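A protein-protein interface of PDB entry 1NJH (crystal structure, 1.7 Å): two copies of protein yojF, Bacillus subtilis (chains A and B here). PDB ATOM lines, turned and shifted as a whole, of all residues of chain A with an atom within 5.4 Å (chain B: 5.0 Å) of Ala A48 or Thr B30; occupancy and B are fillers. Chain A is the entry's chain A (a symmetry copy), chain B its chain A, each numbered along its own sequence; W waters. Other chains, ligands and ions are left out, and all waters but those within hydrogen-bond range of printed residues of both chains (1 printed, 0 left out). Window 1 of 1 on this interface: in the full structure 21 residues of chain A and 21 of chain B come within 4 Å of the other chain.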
ATOM      1  N   LEU A  28       7.782   9.614  12.264  1.00  0.00           N
ATOM      2  CA  LEU A  28       6.550   8.927  12.660  1.00  0.00           C
ATOM      3  C   LEU A  28       5.505   9.382  11.674  1.00  0.00           C
ATOM      4  O   LEU A  28       5.217  10.573  11.574  1.00  0.00           O
ATOM      5  CB  LEU A  28       6.137   9.319  14.075  1.00  0.00           C
ATOM      6  CG  LEU A  28       4.820   8.697  14.559  1.00  0.00           C
ATOM      7  CD1 LEU A  28       4.928   7.177  14.596  1.00  0.00           C
ATOM      8  CD2 LEU A  28       4.475   9.263  15.931  1.00  0.00           C
ATOM      9  N   GLU A  29       4.933   8.431  10.954  1.00  0.00           N
ATOM     10  CA  GLU A  29       3.974   8.759   9.910  1.00  0.00           C
ATOM     11  C   GLU A  29       2.852   7.726   9.804  1.00  0.00           C
ATOM     12  O   GLU A  29       3.068   6.529  10.020  1.00  0.00           O
ATOM     13  CB  GLU A  29       4.752   8.852   8.580  1.00  0.00           C
ATOM     14  CG  GLU A  29       3.907   8.919   7.303  1.00  0.00           C
ATOM     15  CD  GLU A  29       4.754   9.044   6.029  1.00  0.00           C
ATOM     16  OE1 GLU A  29       5.938   8.635   6.033  1.00  0.00           O
ATOM     17  OE2 GLU A  29       4.231   9.545   5.003  1.00  0.00           O
ATOM     18  N   THR A  30       1.656   8.208   9.479  1.00  0.00           N
ATOM     19  CA  THR A  30       0.489   7.345   9.288  1.00  0.00           C
ATOM     20  C   THR A  30      -0.126   7.732   7.949  1.00  0.00           C
ATOM     21  O   THR A  30      -0.265   8.910   7.635  1.00  0.00           O
ATOM     22  CB  THR A  30      -0.586   7.504  10.417  1.00  0.00           C
ATOM     23  OG1 THR A  30      -0.963   8.876  10.564  1.00  0.00           O
ATOM     24  CG2 THR A  30      -0.042   7.006  11.727  1.00  0.00           C
ATOM     25  N   VAL A  46      -1.019  10.760   2.965  1.00  0.00           N
ATOM     26  CA  VAL A  46      -0.450  10.960   4.292  1.00  0.00           C
ATOM     27  C   VAL A  46      -1.506  11.575   5.207  1.00  0.00           C
ATOM     28  O   VAL A  46      -2.257  12.458   4.789  1.00  0.00           O
ATOM     29  CB  VAL A  46       0.781  11.896   4.227  1.00  0.00           C
ATOM     30  CG1 VAL A  46       1.269  12.220   5.631  1.00  0.00           C
ATOM     31  CG2 VAL A  46       1.898  11.230   3.428  1.00  0.00           C
ATOM     32  N   VAL A  47      -1.572  11.099   6.445  1.00  0.00           N
ATOM     33  CA  VAL A  47      -2.536  11.615   7.415  1.00  0.00           C
ATOM     34  C   VAL A  47      -1.816  12.477   8.458  1.00  0.00           C
ATOM     35  O   VAL A  47      -2.129  13.657   8.623  1.00  0.00           O
ATOM     36  CB  VAL A  47      -3.285  10.448   8.127  1.00  0.00           C
ATOM     37  CG1 VAL A  47      -4.162  10.974   9.270  1.00  0.00           C
ATOM     38  CG2 VAL A  47      -4.142   9.700   7.111  1.00  0.00           C
ATOM     39  N   ALA A  48      -0.863  11.881   9.163  1.00  0.00           N
ATOM     40  CA  ALA A  48      -0.095  12.592  10.184  1.00  0.00           C
ATOM     41  C   ALA A  48       1.360  12.299   9.909  1.00  0.00           C
ATOM     42  O   ALA A  48       1.724  11.174   9.563  1.00  0.00           O
ATOM     43  CB  ALA A  48      -0.466  12.117  11.585  1.00  0.00           C
ATOM     44  N   TYR A  49       2.206  13.292  10.135  1.00  0.00           N
ATOM     45  CA  TYR A  49       3.594  13.132   9.802  1.00  0.00           C
ATOM     46  C   TYR A  49       4.500  14.007  10.658  1.00  0.00           C
ATOM     47  O   TYR A  49       4.269  15.212  10.777  1.00  0.00           O
ATOM     48  CB  TYR A  49       3.678  13.527   8.315  1.00  0.00           C
ATOM     49  CG  TYR A  49       5.004  13.498   7.609  1.00  0.00           C
ATOM     50  CD1 TYR A  49       5.302  12.469   6.715  1.00  0.00           C
ATOM     51  CD2 TYR A  49       5.908  14.558   7.726  1.00  0.00           C
ATOM     52  CE1 TYR A  49       6.467  12.492   5.939  1.00  0.00           C
ATOM     53  CE2 TYR A  49       7.077  14.596   6.952  1.00  0.00           C
ATOM     54  CZ  TYR A  49       7.345  13.558   6.060  1.00  0.00           C
ATOM     55  OH  TYR A  49       8.477  13.578   5.274  1.00  0.00           O
ATOM     56  N   ILE A  50       5.489  13.403  11.307  1.00  0.00           N
ATOM     57  CA  ILE A  50       6.486  14.208  12.006  1.00  0.00           C
ATOM     58  C   ILE A  50       7.814  13.618  11.528  1.00  0.00           C
ATOM     59  O   ILE A  50       8.058  12.419  11.642  1.00  0.00           O
ATOM     60  CB  ILE A  50       6.345  14.234  13.556  1.00  0.00           C
ATOM     61  CG1 ILE A  50       7.336  15.275  14.109  1.00  0.00           C
ATOM     62  CG2 ILE A  50       6.567  12.860  14.153  1.00  0.00           C
ATOM     63  CD1 ILE A  50       7.097  15.727  15.540  1.00  0.00           C
ATOM     64  N   LEU B  28       0.143  15.449  18.563  1.00  0.00           N
ATOM     65  CA  LEU B  28      -0.256  15.024  17.220  1.00  0.00           C
ATOM     66  C   LEU B  28      -0.662  13.580  17.362  1.00  0.00           C
ATOM     67  O   LEU B  28       0.143  12.741  17.762  1.00  0.00           O
ATOM     68  CB  LEU B  28       0.907  15.144  16.240  1.00  0.00           C
ATOM     69  CG  LEU B  28       0.605  14.661  14.815  1.00  0.00           C
ATOM     70  CD1 LEU B  28      -0.509  15.496  14.193  1.00  0.00           C
ATOM     71  CD2 LEU B  28       1.879  14.730  13.984  1.00  0.00           C
ATOM     72  N   GLU B  29      -1.909  13.292  17.026  1.00  0.00           N
ATOM     73  CA  GLU B  29      -2.439  11.949  17.204  1.00  0.00           C
ATOM     74  C   GLU B  29      -3.412  11.552  16.093  1.00  0.00           C
ATOM     75  O   GLU B  29      -4.154  12.391  15.571  1.00  0.00           O
ATOM     76  CB  GLU B  29      -3.140  11.907  18.578  1.00  0.00           C
ATOM     77  CG  GLU B  29      -4.006  10.673  18.861  1.00  0.00           C
ATOM     78  CD  GLU B  29      -4.640  10.694  20.260  1.00  0.00           C
ATOM     79  OE1 GLU B  29      -4.816  11.789  20.841  1.00  0.00           O
ATOM     80  OE2 GLU B  29      -4.981   9.605  20.783  1.00  0.00           O
ATOM     81  N   THR B  30      -3.387  10.272  15.737  1.00  0.00           N
ATOM     82  CA  THR B  30      -4.291   9.723  14.724  1.00  0.00           C
ATOM     83  C   THR B  30      -4.930   8.482  15.336  1.00  0.00           C
ATOM     84  O   THR B  30      -4.256   7.668  15.961  1.00  0.00           O
ATOM     85  CB  THR B  30      -3.561   9.329  13.396  1.00  0.00           C
ATOM     86  OG1 THR B  30      -2.469   8.445  13.664  1.00  0.00           O
ATOM     87  CG2 THR B  30      -3.033  10.558  12.708  1.00  0.00           C
ATOM     88  N   THR B  31      -6.235   8.349  15.149  1.00  0.00           N
ATOM     89  CA  THR B  31      -6.978   7.218  15.700  1.00  0.00           C
ATOM     90  C   THR B  31      -7.862   6.603  14.620  1.00  0.00           C
ATOM     91  O   THR B  31      -8.126   7.234  13.599  1.00  0.00           O
ATOM     92  CB  THR B  31      -7.875   7.678  16.853  1.00  0.00           C
ATOM     93  OG1 THR B  31      -8.717   8.742  16.392  1.00  0.00           O
ATOM     94  CG2 THR B  31      -7.036   8.178  18.021  1.00  0.00           C
ATOM     95  N   THR B  32      -8.319   5.374  14.853  1.00  0.00           N
ATOM     96  CA  THR B  32      -9.182   4.685  13.896  1.00  0.00           C
ATOM     97  C   THR B  32     -10.197   3.797  14.603  1.00  0.00           C
ATOM     98  O   THR B  32     -10.185   3.674  15.829  1.00  0.00           O
ATOM     99  CB  THR B  32      -8.375   3.793  12.934  1.00  0.00           C
ATOM    100  OG1 THR B  32      -7.753   2.732  13.669  1.00  0.00           O
ATOM    101  CG2 THR B  32      -7.310   4.609  12.226  1.00  0.00           C
ATOM    102  N   THR B  45      -9.345   3.321  18.518  1.00  0.00           N
ATOM    103  CA  THR B  45      -7.999   2.889  18.876  1.00  0.00           C
ATOM    104  C   THR B  45      -6.946   3.874  18.372  1.00  0.00           C
ATOM    105  O   THR B  45      -7.040   4.380  17.253  1.00  0.00           O
ATOM    106  CB  THR B  45      -7.694   1.492  18.298  1.00  0.00           C
ATOM    107  OG1 THR B  45      -7.828   1.522  16.873  1.00  0.00           O
ATOM    108  CG2 THR B  45      -8.656   0.465  18.872  1.00  0.00           C
ATOM    109  N   VAL B  46      -5.951   4.149  19.208  1.00  0.00           N
ATOM    110  CA  VAL B  46      -4.881   5.066  18.833  1.00  0.00           C
ATOM    111  C   VAL B  46      -3.941   4.372  17.850  1.00  0.00           C
ATOM    112  O   VAL B  46      -3.625   3.192  18.015  1.00  0.00           O
ATOM    113  CB  VAL B  46      -4.080   5.515  20.078  1.00  0.00           C
ATOM    114  CG1 VAL B  46      -2.876   6.345  19.657  1.00  0.00           C
ATOM    115  CG2 VAL B  46      -4.977   6.332  21.006  1.00  0.00           C
ATOM    116  N   VAL B  47      -3.510   5.096  16.824  1.00  0.00           N
ATOM    117  CA  VAL B  47      -2.601   4.543  15.823  1.00  0.00           C
ATOM    118  C   VAL B  47      -1.197   5.129  16.013  1.00  0.00           C
ATOM    119  O   VAL B  47      -0.232   4.395  16.227  1.00  0.00           O
ATOM    120  CB  VAL B  47      -3.106   4.855  14.381  1.00  0.00           C
ATOM    121  CG1 VAL B  47      -2.068   4.440  13.333  1.00  0.00           C
ATOM    122  CG2 VAL B  47      -4.421   4.123  14.135  1.00  0.00           C
ATOM    123  N   ALA B  48      -1.089   6.449  15.925  1.00  0.00           N
ATOM    124  CA  ALA B  48       0.192   7.134  16.094  1.00  0.00           C
ATOM    125  C   ALA B  48      -0.048   8.256  17.076  1.00  0.00           C
ATOM    126  O   ALA B  48      -1.083   8.924  17.032  1.00  0.00           O
ATOM    127  CB  ALA B  48       0.695   7.700  14.770  1.00  0.00           C
ATOM    128  N   TYR B  80       3.332  17.655   9.964  1.00  0.00           N
ATOM    129  CA  TYR B  80       2.280  17.792   8.978  1.00  0.00           C
ATOM    130  C   TYR B  80       1.038  16.992   9.370  1.00  0.00           C
ATOM    131  O   TYR B  80       1.141  15.871   9.874  1.00  0.00           O
ATOM    132  CB  TYR B  80       2.839  17.309   7.643  1.00  0.00           C
ATOM    133  CG  TYR B  80       1.864  17.268   6.507  1.00  0.00           C
ATOM    134  CD1 TYR B  80       1.549  18.418   5.784  1.00  0.00           C
ATOM    135  CD2 TYR B  80       1.272  16.067   6.131  1.00  0.00           C
ATOM    136  CE1 TYR B  80       0.662  18.364   4.710  1.00  0.00           C
ATOM    137  CE2 TYR B  80       0.390  16.002   5.063  1.00  0.00           C
ATOM    138  CZ  TYR B  80       0.088  17.149   4.357  1.00  0.00           C
ATOM    139  OH  TYR B  80      -0.796  17.066   3.296  1.00  0.00           O
ATOM    140  N   ALA B  81      -0.134  17.592   9.166  1.00  0.00           N
ATOM    141  CA  ALA B  81      -1.407  16.944   9.489  1.00  0.00           C
ATOM    142  C   ALA B  81      -2.413  17.283   8.390  1.00  0.00           C
ATOM    143  O   ALA B  81      -2.576  18.449   8.028  1.00  0.00           O
ATOM    144  CB  ALA B  81      -1.938  17.434  10.844  1.00  0.00           C
ATOM    145  N   LEU B 106     -11.608   7.590  10.523  1.00  0.00           N
ATOM    146  CA  LEU B 106     -10.262   8.080  10.776  1.00  0.00           C
ATOM    147  C   LEU B 106     -10.377   9.423  11.482  1.00  0.00           C
ATOM    148  O   LEU B 106     -11.216  10.247  11.130  1.00  0.00           O
ATOM    149  CB  LEU B 106      -9.506   8.256   9.461  1.00  0.00           C
ATOM    150  CG  LEU B 106      -8.001   7.965   9.449  1.00  0.00           C
ATOM    151  CD1 LEU B 106      -7.418   8.546   8.167  1.00  0.00           C
ATOM    152  CD2 LEU B 106      -7.309   8.572  10.660  1.00  0.00           C
ATOM    153  N   ALA B 107      -9.542   9.640  12.488  1.00  0.00           N
ATOM    154  CA  ALA B 107      -9.573  10.896  13.209  1.00  0.00           C
ATOM    155  C   ALA B 107      -8.164  11.409  13.403  1.00  0.00           C
ATOM    156  O   ALA B 107      -7.199  10.630  13.484  1.00  0.00           O
ATOM    157  CB  ALA B 107     -10.251  10.720  14.567  1.00  0.00           C
ATOM    158  N   ILE B 108      -8.051  12.726  13.479  1.00  0.00           N
ATOM    159  CA  ILE B 108      -6.758  13.348  13.664  1.00  0.00           C
ATOM    160  C   ILE B 108      -6.864  14.558  14.564  1.00  0.00           C
ATOM    161  O   ILE B 108      -7.891  15.241  14.607  1.00  0.00           O
ATOM    162  CB  ILE B 108      -6.145  13.760  12.317  1.00  0.00           C
ATOM    163  CG1 ILE B 108      -4.764  14.375  12.550  1.00  0.00           C
ATOM    164  CG2 ILE B 108      -7.088  14.730  11.591  1.00  0.00           C
ATOM    165  CD1 ILE B 108      -3.910  14.409  11.322  1.00  0.00           C
HETATM  166  O   HOH W   1      -2.382  14.647   2.977  1.00  0.00           O
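Water W1 bridges the backbone carbonyl oxygen (O) of Val A46 (2.8 Å) and the side-chain hydroxyl (OH) of Tyr B80 (2.9 Å).
Among the printed residues, merely in contact across the chains: Thr A30 with Val B47, Thr A30 with Ala B48, Val A46 with Tyr B80, Val A47 with Thr B30, Val A47 with Ala B81, Val A47 with Leu B106, Val A47 with Ile B108, Ala A48 with Thr B30 and Ala A48 with Tyr B80.
Printed residues of chain A that touch a printed residue of chain B: Thr A30, Val A46, Val A47, Ala A48 and Tyr A49.
Hydrophobic or aromatic side chains of chain A within 4 Å of the printed part of chain B: Val A46, Val A47, Ala A48 and Tyr A49.
Among the printed residues, no Asp or Glu carboxylate lies within 4 Å of a Lys or Arg side-chain nitrogen of the other chain.
The side-chain hydroxyl (OG1) of Thr A30 lies close to the side-chain hydroxyl (OG1) of Thr B30 (3.5 Å).
O of Tyr A49 lies within hydrogen-bond range of N of Tyr B80 (2.7 Å).
Thr B30 touches its own counterpart, Thr A30.
Thr A30 touches Val B47, and with the chains exchanged Val A47 touches Thr B30.
Thr A30 touches Ala B48, and with the chains exchanged Ala A48 touches Thr B30.
Of the 11 pairs that touch across the chains among the printed residues, 5 have their exchanged pair printed and touching as well.
O of Thr B30 sits at hydrogen-bond distance from N of Val B47 (2.8 Å).
The backbone NH (N) of Thr B30 is in hydrogen-bond range of the backbone carbonyl oxygen (O) of Ala B48 (3.0 Å).
N of Val A47 lies within hydrogen-bond range of O of Thr A30, at 2.8 Å.
The backbone NH (N) of Thr A30 is in hydrogen-bond range of the backbone carbonyl oxygen (O) of Ala A48.
Ala A48 touches two residues of chain B.
Thr B30 touches three residues of chain A.
Of the printed residues of chain A, Ala B81 touches Val A47.
Printed residues of chain B within 4 Å of Tyr A49: Tyr B80.
Printed residues of chain A within 4 Å of Ile B108: Val A47 (3.3 Å).
Ile A50 touches none of the printed residues of chain B.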
